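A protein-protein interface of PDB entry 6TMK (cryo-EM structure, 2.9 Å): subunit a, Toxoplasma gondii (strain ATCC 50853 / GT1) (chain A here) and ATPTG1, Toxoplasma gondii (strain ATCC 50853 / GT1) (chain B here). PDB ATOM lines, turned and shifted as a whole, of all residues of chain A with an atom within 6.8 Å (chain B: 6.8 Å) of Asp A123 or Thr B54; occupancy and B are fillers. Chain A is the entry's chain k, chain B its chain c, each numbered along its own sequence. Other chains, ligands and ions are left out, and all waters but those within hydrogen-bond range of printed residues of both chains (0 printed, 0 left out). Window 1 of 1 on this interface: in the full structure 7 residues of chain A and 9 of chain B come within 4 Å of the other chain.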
ATOM      1  N   GLN A 118      -0.860  -1.354   9.510  1.00  0.00           N
ATOM      2  CA  GLN A 118      -0.172  -0.684   8.415  1.00  0.00           C
ATOM      3  C   GLN A 118      -0.995   0.525   8.003  1.00  0.00           C
ATOM      4  O   GLN A 118      -2.181   0.394   7.693  1.00  0.00           O
ATOM      5  CB  GLN A 118       0.031  -1.624   7.221  1.00  0.00           C
ATOM      6  CG  GLN A 118       0.695  -2.944   7.576  1.00  0.00           C
ATOM      7  CD  GLN A 118       2.169  -2.794   7.898  1.00  0.00           C
ATOM      8  OE1 GLN A 118       2.619  -1.730   8.323  1.00  0.00           O
ATOM      9  NE2 GLN A 118       2.928  -3.864   7.701  1.00  0.00           N
ATOM     10  N   THR A 119      -0.364   1.696   8.000  1.00  0.00           N
ATOM     11  CA  THR A 119      -1.064   2.967   7.932  1.00  0.00           C
ATOM     12  C   THR A 119      -0.728   3.692   6.636  1.00  0.00           C
ATOM     13  O   THR A 119       0.218   3.347   5.923  1.00  0.00           O
ATOM     14  CB  THR A 119      -0.708   3.850   9.134  1.00  0.00           C
ATOM     15  OG1 THR A 119       0.711   4.043   9.184  1.00  0.00           O
ATOM     16  CG2 THR A 119      -1.170   3.197  10.425  1.00  0.00           C
ATOM     17  N   SER A 120      -1.525   4.714   6.341  1.00  0.00           N
ATOM     18  CA  SER A 120      -1.277   5.614   5.227  1.00  0.00           C
ATOM     19  C   SER A 120      -0.331   6.739   5.637  1.00  0.00           C
ATOM     20  O   SER A 120      -0.140   7.029   6.821  1.00  0.00           O
ATOM     21  CB  SER A 120      -2.590   6.201   4.709  1.00  0.00           C
ATOM     22  OG  SER A 120      -2.353   7.340   3.900  1.00  0.00           O
ATOM     23  N   LEU A 121       0.261   7.378   4.626  1.00  0.00           N
ATOM     24  CA  LEU A 121       1.017   8.603   4.861  1.00  0.00           C
ATOM     25  C   LEU A 121       0.151   9.650   5.552  1.00  0.00           C
ATOM     26  O   LEU A 121       0.576  10.281   6.527  1.00  0.00           O
ATOM     27  CB  LEU A 121       1.561   9.139   3.537  1.00  0.00           C
ATOM     28  CG  LEU A 121       2.569  10.289   3.609  1.00  0.00           C
ATOM     29  CD1 LEU A 121       3.489  10.250   2.400  1.00  0.00           C
ATOM     30  CD2 LEU A 121       1.879  11.642   3.702  1.00  0.00           C
ATOM     31  N   ALA A 122      -1.065   9.864   5.045  1.00  0.00           N
ATOM     32  CA  ALA A 122      -1.958  10.835   5.666  1.00  0.00           C
ATOM     33  C   ALA A 122      -2.375  10.387   7.061  1.00  0.00           C
ATOM     34  O   ALA A 122      -2.499  11.212   7.972  1.00  0.00           O
ATOM     35  CB  ALA A 122      -3.187  11.055   4.785  1.00  0.00           C
ATOM     36  N   ASP A 123      -2.577   9.082   7.250  1.00  0.00           N
ATOM     37  CA  ASP A 123      -2.880   8.559   8.579  1.00  0.00           C
ATOM     38  C   ASP A 123      -1.780   8.920   9.568  1.00  0.00           C
ATOM     39  O   ASP A 123      -2.051   9.413  10.670  1.00  0.00           O
ATOM     40  CB  ASP A 123      -3.069   7.042   8.518  1.00  0.00           C
ATOM     41  CG  ASP A 123      -4.492   6.642   8.167  1.00  0.00           C
ATOM     42  OD1 ASP A 123      -4.679   5.527   7.635  1.00  0.00           O
ATOM     43  OD2 ASP A 123      -5.422   7.434   8.424  1.00  0.00           O
ATOM     44  N   LYS A 124      -0.525   8.685   9.188  1.00  0.00           N
ATOM     45  CA  LYS A 124       0.567   8.910  10.125  1.00  0.00           C
ATOM     46  C   LYS A 124       0.869  10.392  10.294  1.00  0.00           C
ATOM     47  O   LYS A 124       1.305  10.805  11.372  1.00  0.00           O
ATOM     48  CB  LYS A 124       1.812   8.149   9.669  1.00  0.00           C
ATOM     49  CG  LYS A 124       2.452   8.672   8.399  1.00  0.00           C
ATOM     50  CD  LYS A 124       3.685   7.856   8.039  1.00  0.00           C
ATOM     51  CE  LYS A 124       3.310   6.487   7.488  1.00  0.00           C
ATOM     52  NZ  LYS A 124       4.502   5.656   7.163  1.00  0.00           N
ATOM     53  N   THR A 125       0.607  11.213   9.276  1.00  0.00           N
ATOM     54  CA  THR A 125       0.667  12.658   9.475  1.00  0.00           C
ATOM     55  C   THR A 125      -0.383  13.108  10.483  1.00  0.00           C
ATOM     56  O   THR A 125      -0.099  13.919  11.376  1.00  0.00           O
ATOM     57  CB  THR A 125       0.473  13.383   8.143  1.00  0.00           C
ATOM     58  OG1 THR A 125       1.468  12.951   7.208  1.00  0.00           O
ATOM     59  CG2 THR A 125       0.576  14.890   8.333  1.00  0.00           C
ATOM     60  N   ARG A 126      -1.606  12.591  10.350  1.00  0.00           N
ATOM     61  CA  ARG A 126      -2.676  12.957  11.270  1.00  0.00           C
ATOM     62  C   ARG A 126      -2.345  12.516  12.688  1.00  0.00           C
ATOM     63  O   ARG A 126      -2.660  13.216  13.656  1.00  0.00           O
ATOM     64  CB  ARG A 126      -3.988  12.330  10.803  1.00  0.00           C
ATOM     65  CG  ARG A 126      -5.229  13.092  11.203  1.00  0.00           C
ATOM     66  CD  ARG A 126      -6.420  12.639  10.381  1.00  0.00           C
ATOM     67  NE  ARG A 126      -6.690  11.215  10.550  1.00  0.00           N
ATOM     68  CZ  ARG A 126      -7.483  10.502   9.756  1.00  0.00           C
ATOM     69  NH1 ARG A 126      -8.093  11.076   8.726  1.00  0.00           N
ATOM     70  NH2 ARG A 126      -7.666   9.211   9.990  1.00  0.00           N
ATOM     71  N   GLY A 127      -1.696  11.359  12.827  1.00  0.00           N
ATOM     72  CA  GLY A 127      -1.292  10.908  14.149  1.00  0.00           C
ATOM     73  C   GLY A 127      -0.162  11.739  14.725  1.00  0.00           C
ATOM     74  O   GLY A 127      -0.160  12.060  15.917  1.00  0.00           O
ATOM     75  N   LEU A 128       0.814  12.099  13.889  1.00  0.00           N
ATOM     76  CA  LEU A 128       1.870  13.011  14.313  1.00  0.00           C
ATOM     77  C   LEU A 128       1.285  14.311  14.843  1.00  0.00           C
ATOM     78  O   LEU A 128       1.719  14.821  15.882  1.00  0.00           O
ATOM     79  CB  LEU A 128       2.817  13.286  13.147  1.00  0.00           C
ATOM     80  CG  LEU A 128       4.167  13.917  13.494  1.00  0.00           C
ATOM     81  CD1 LEU A 128       5.220  13.461  12.502  1.00  0.00           C
ATOM     82  CD2 LEU A 128       4.080  15.434  13.517  1.00  0.00           C
ATOM     83  N   GLY A 130      -1.743  14.655  15.986  1.00  0.00           N
ATOM     84  CA  GLY A 130      -2.634  14.366  17.091  1.00  0.00           C
ATOM     85  C   GLY A 130      -3.967  15.070  16.967  1.00  0.00           C
ATOM     86  O   GLY A 130      -4.287  15.964  17.755  1.00  0.00           O
ATOM     87  N   VAL A 131      -4.755  14.669  15.970  1.00  0.00           N
ATOM     88  CA  VAL A 131      -6.034  15.328  15.719  1.00  0.00           C
ATOM     89  C   VAL A 131      -7.021  15.011  16.836  1.00  0.00           C
ATOM     90  O   VAL A 131      -7.501  15.907  17.540  1.00  0.00           O
ATOM     91  CB  VAL A 131      -6.585  14.918  14.342  1.00  0.00           C
ATOM     92  CG1 VAL A 131      -8.075  15.205  14.247  1.00  0.00           C
ATOM     93  CG2 VAL A 131      -5.827  15.638  13.241  1.00  0.00           C
ATOM     94  N   GLY A 132      -7.337  13.729  17.013  1.00  0.00           N
ATOM     95  CA  GLY A 132      -8.356  13.325  17.958  1.00  0.00           C
ATOM     96  C   GLY A 132      -7.815  12.987  19.332  1.00  0.00           C
ATOM     97  O   GLY A 132      -8.482  12.298  20.110  1.00  0.00           O
ATOM     98  N   PHE A 133      -6.608  13.464  19.645  1.00  0.00           N
ATOM     99  CA  PHE A 133      -5.949  13.121  20.897  1.00  0.00           C
ATOM    100  C   PHE A 133      -5.331  14.308  21.621  1.00  0.00           C
ATOM    101  O   PHE A 133      -4.915  14.148  22.774  1.00  0.00           O
ATOM    102  CB  PHE A 133      -4.852  12.075  20.654  1.00  0.00           C
ATOM    103  CG  PHE A 133      -5.298  10.914  19.814  1.00  0.00           C
ATOM    104  CD1 PHE A 133      -6.037   9.884  20.370  1.00  0.00           C
ATOM    105  CD2 PHE A 133      -4.983  10.854  18.468  1.00  0.00           C
ATOM    106  CE1 PHE A 133      -6.453   8.818  19.602  1.00  0.00           C
ATOM    107  CE2 PHE A 133      -5.394   9.788  17.695  1.00  0.00           C
ATOM    108  CZ  PHE A 133      -6.130   8.769  18.264  1.00  0.00           C
ATOM    109  N   VAL B  49     -12.866   3.532  12.277  1.00  0.00           N
ATOM    110  CA  VAL B  49     -11.711   2.926  11.618  1.00  0.00           C
ATOM    111  C   VAL B  49     -10.619   3.969  11.429  1.00  0.00           C
ATOM    112  O   VAL B  49      -9.433   3.716  11.684  1.00  0.00           O
ATOM    113  CB  VAL B  49     -12.122   2.290  10.280  1.00  0.00           C
ATOM    114  CG1 VAL B  49     -10.890   1.879   9.494  1.00  0.00           C
ATOM    115  CG2 VAL B  49     -13.014   1.093  10.523  1.00  0.00           C
ATOM    116  N   ALA B  50     -11.004   5.143  10.929  1.00  0.00           N
ATOM    117  CA  ALA B  50     -10.036   6.222  10.750  1.00  0.00           C
ATOM    118  C   ALA B  50      -9.366   6.566  12.075  1.00  0.00           C
ATOM    119  O   ALA B  50      -8.138   6.737  12.145  1.00  0.00           O
ATOM    120  CB  ALA B  50     -10.726   7.447  10.155  1.00  0.00           C
ATOM    121  N   LEU B  51     -10.165   6.665  13.141  1.00  0.00           N
ATOM    122  CA  LEU B  51      -9.630   6.989  14.455  1.00  0.00           C
ATOM    123  C   LEU B  51      -8.648   5.920  14.909  1.00  0.00           C
ATOM    124  O   LEU B  51      -7.605   6.231  15.487  1.00  0.00           O
ATOM    125  CB  LEU B  51     -10.770   7.134  15.461  1.00  0.00           C
ATOM    126  CG  LEU B  51     -10.374   7.434  16.906  1.00  0.00           C
ATOM    127  CD1 LEU B  51      -9.491   8.667  16.992  1.00  0.00           C
ATOM    128  CD2 LEU B  51     -11.611   7.605  17.768  1.00  0.00           C
ATOM    129  N   ASN B  52      -8.968   4.653  14.653  1.00  0.00           N
ATOM    130  CA  ASN B  52      -8.100   3.566  15.087  1.00  0.00           C
ATOM    131  C   ASN B  52      -6.782   3.591  14.329  1.00  0.00           C
ATOM    132  O   ASN B  52      -5.718   3.345  14.909  1.00  0.00           O
ATOM    133  CB  ASN B  52      -8.803   2.228  14.887  1.00  0.00           C
ATOM    134  CG  ASN B  52      -8.034   1.076  15.484  1.00  0.00           C
ATOM    135  OD1 ASN B  52      -7.063   1.272  16.211  1.00  0.00           O
ATOM    136  ND2 ASN B  52      -8.461  -0.137  15.174  1.00  0.00           N
ATOM    137  N   ARG B  53      -6.833   3.869  13.027  1.00  0.00           N
ATOM    138  CA  ARG B  53      -5.606   3.937  12.241  1.00  0.00           C
ATOM    139  C   ARG B  53      -4.710   5.067  12.733  1.00  0.00           C
ATOM    140  O   ARG B  53      -3.502   4.877  12.936  1.00  0.00           O
ATOM    141  CB  ARG B  53      -5.933   4.113  10.761  1.00  0.00           C
ATOM    142  CG  ARG B  53      -6.565   2.897  10.121  1.00  0.00           C
ATOM    143  CD  ARG B  53      -6.890   3.153   8.661  1.00  0.00           C
ATOM    144  NE  ARG B  53      -7.677   2.074   8.077  1.00  0.00           N
ATOM    145  CZ  ARG B  53      -8.309   2.155   6.910  1.00  0.00           C
ATOM    146  NH1 ARG B  53      -8.249   3.270   6.194  1.00  0.00           N
ATOM    147  NH2 ARG B  53      -9.001   1.119   6.460  1.00  0.00           N
ATOM    148  N   THR B  54      -5.287   6.252  12.951  1.00  0.00           N
ATOM    149  CA  THR B  54      -4.465   7.348  13.450  1.00  0.00           C
ATOM    150  C   THR B  54      -3.985   7.076  14.870  1.00  0.00           C
ATOM    151  O   THR B  54      -2.900   7.523  15.250  1.00  0.00           O
ATOM    152  CB  THR B  54      -5.228   8.670  13.392  1.00  0.00           C
ATOM    153  OG1 THR B  54      -4.374   9.735  13.829  1.00  0.00           O
ATOM    154  CG2 THR B  54      -6.453   8.624  14.269  1.00  0.00           C
ATOM    155  N   PHE B  55      -4.768   6.344  15.661  1.00  0.00           N
ATOM    156  CA  PHE B  55      -4.350   5.966  17.006  1.00  0.00           C
ATOM    157  C   PHE B  55      -3.118   5.071  16.958  1.00  0.00           C
ATOM    158  O   PHE B  55      -2.124   5.311  17.657  1.00  0.00           O
ATOM    159  CB  PHE B  55      -5.522   5.271  17.701  1.00  0.00           C
ATOM    160  CG  PHE B  55      -5.159   4.540  18.952  1.00  0.00           C
ATOM    161  CD1 PHE B  55      -4.992   5.214  20.144  1.00  0.00           C
ATOM    162  CD2 PHE B  55      -5.024   3.166  18.944  1.00  0.00           C
ATOM    163  CE1 PHE B  55      -4.675   4.532  21.298  1.00  0.00           C
ATOM    164  CE2 PHE B  55      -4.710   2.482  20.091  1.00  0.00           C
ATOM    165  CZ  PHE B  55      -4.533   3.165  21.270  1.00  0.00           C
ATOM    166  N   GLN B  56      -3.171   4.028  16.128  1.00  0.00           N
ATOM    167  CA  GLN B  56      -2.013   3.164  15.929  1.00  0.00           C
ATOM    168  C   GLN B  56      -0.802   3.973  15.494  1.00  0.00           C
ATOM    169  O   GLN B  56       0.312   3.773  15.997  1.00  0.00           O
ATOM    170  CB  GLN B  56      -2.327   2.096  14.883  1.00  0.00           C
ATOM    171  CG  GLN B  56      -3.404   1.121  15.279  1.00  0.00           C
ATOM    172  CD  GLN B  56      -3.900   0.309  14.105  1.00  0.00           C
ATOM    173  OE1 GLN B  56      -3.142  -0.007  13.190  1.00  0.00           O
ATOM    174  NE2 GLN B  56      -5.183  -0.025  14.118  1.00  0.00           N
ATOM    175  N   ALA B  57      -0.994   4.876  14.532  1.00  0.00           N
ATOM    176  CA  ALA B  57       0.141   5.615  13.995  1.00  0.00           C
ATOM    177  C   ALA B  57       0.737   6.530  15.054  1.00  0.00           C
ATOM    178  O   ALA B  57       1.958   6.564  15.244  1.00  0.00           O
ATOM    179  CB  ALA B  57      -0.290   6.420  12.773  1.00  0.00           C
ATOM    180  N   ARG B  58      -0.114   7.283  15.751  1.00  0.00           N
ATOM    181  CA  ARG B  58       0.342   8.118  16.853  1.00  0.00           C
ATOM    182  C   ARG B  58       1.171   7.315  17.838  1.00  0.00           C
ATOM    183  O   ARG B  58       2.302   7.687  18.169  1.00  0.00           O
ATOM    184  CB  ARG B  58      -0.858   8.741  17.561  1.00  0.00           C
ATOM    185  CG  ARG B  58      -0.489   9.580  18.762  1.00  0.00           C
ATOM    186  CD  ARG B  58      -1.690  10.308  19.314  1.00  0.00           C
ATOM    187  NE  ARG B  58      -2.620   9.389  19.965  1.00  0.00           N
ATOM    188  CZ  ARG B  58      -2.715   9.209  21.280  1.00  0.00           C
ATOM    189  NH1 ARG B  58      -1.934   9.877  22.117  1.00  0.00           N
ATOM    190  NH2 ARG B  58      -3.597   8.346  21.761  1.00  0.00           N
ATOM    191  N   ASN B  59       0.628   6.193  18.307  1.00  0.00           N
ATOM    192  CA  ASN B  59       1.354   5.384  19.274  1.00  0.00           C
ATOM    193  C   ASN B  59       2.712   4.975  18.729  1.00  0.00           C
ATOM    194  O   ASN B  59       3.750   5.442  19.212  1.00  0.00           O
ATOM    195  CB  ASN B  59       0.534   4.157  19.653  1.00  0.00           C
ATOM    196  CG  ASN B  59      -0.303   4.377  20.889  1.00  0.00           C
ATOM    197  OD1 ASN B  59       0.156   4.169  22.010  1.00  0.00           O
ATOM    198  ND2 ASN B  59      -1.538   4.804  20.693  1.00  0.00           N
ATOM    199  N   LEU B  61       4.541   5.773  16.276  1.00  0.00           N
ATOM    200  CA  LEU B  61       5.503   6.800  15.896  1.00  0.00           C
ATOM    201  C   LEU B  61       6.034   7.537  17.120  1.00  0.00           C
ATOM    202  O   LEU B  61       7.236   7.508  17.403  1.00  0.00           O
ATOM    203  CB  LEU B  61       4.862   7.792  14.924  1.00  0.00           C
ATOM    204  CG  LEU B  61       4.692   7.357  13.470  1.00  0.00           C
ATOM    205  CD1 LEU B  61       4.036   8.471  12.687  1.00  0.00           C
ATOM    206  CD2 LEU B  61       6.019   6.976  12.839  1.00  0.00           C
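The backbone carbonyl oxygen (O) of Ala B50 lies within hydrogen-bond range of the guanidinium group (NH2) of Arg A126.
OG1 of Thr B54 is in hydrogen-bond range of N of Gly A127 (3.3 Å).
O of Phe B55 sits at hydrogen-bond distance from ND2 of Asn B59.
The side-chain carboxylate (OD2) of Asp A123 is in salt-bridge range of the guanidinium group (NH2) of Arg A126.
The backbone carbonyl oxygen of Arg A126 sits at hydrogen-bond distance from the backbone NH of Val A131.
CG2 of Thr A119 touches O of Arg B53, at 3.8 Å.
Arg B53 touches Asp A123.
Thr B54 touches Asp A123.
CB of Ala B57 touches CA of Lys A124, 3.7 Å away.
Thr B54 touches Arg A126.
Gly A127 touches Arg B58.
Phe A133 touches Leu B51.
Phe A133 touches Thr B54.
Phe A133 touches Phe B55 (CZ to CA, 3.6 Å).
Phe A133 touches Arg B58.
Asp A123 touches just these residues of chain B: Arg B53 and Thr B54.
Thr B54 touches just these residues of chain A: Asp A123, Arg A126, Gly A127 and Phe A133.
Of the printed residues of chain B, Lys A124 touches Ala B57 (3.7 Å) and Leu B61 (3.8 Å).
Of the printed residues of chain A, Arg B58 touches Gly A127 (3.8 Å) and Phe A133 (3.1 Å).
Of the printed residues of chain B, Phe A133 touches Leu B51 (3.6 Å), Thr B54 (3.8 Å), Phe B55 (3.6 Å) and Arg B58 (3.1 Å).
Printed residues of chain A within 4 Å of Leu B61: Lys A124.
Of the printed residues of chain A, Leu B51 touches Phe A133.
Val B49 touches none of the printed residues of chain A.
Gly A130 touches none of the printed residues of chain B.
The nearest residue of chain B that does not touch Asp A123 is Ala B57 (4.1 Å).
The nearest residue of chain A that does not touch Thr B54 is Val A131 (5.4 Å).
Of the 12 printed residues of chain B, 8 touch a printed residue of chain A.
Hydrophobic or aromatic side chains of chain B that line the printed part of chain A: Ala B50, Leu B51, Phe B55, Ala B57 and Leu B61.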
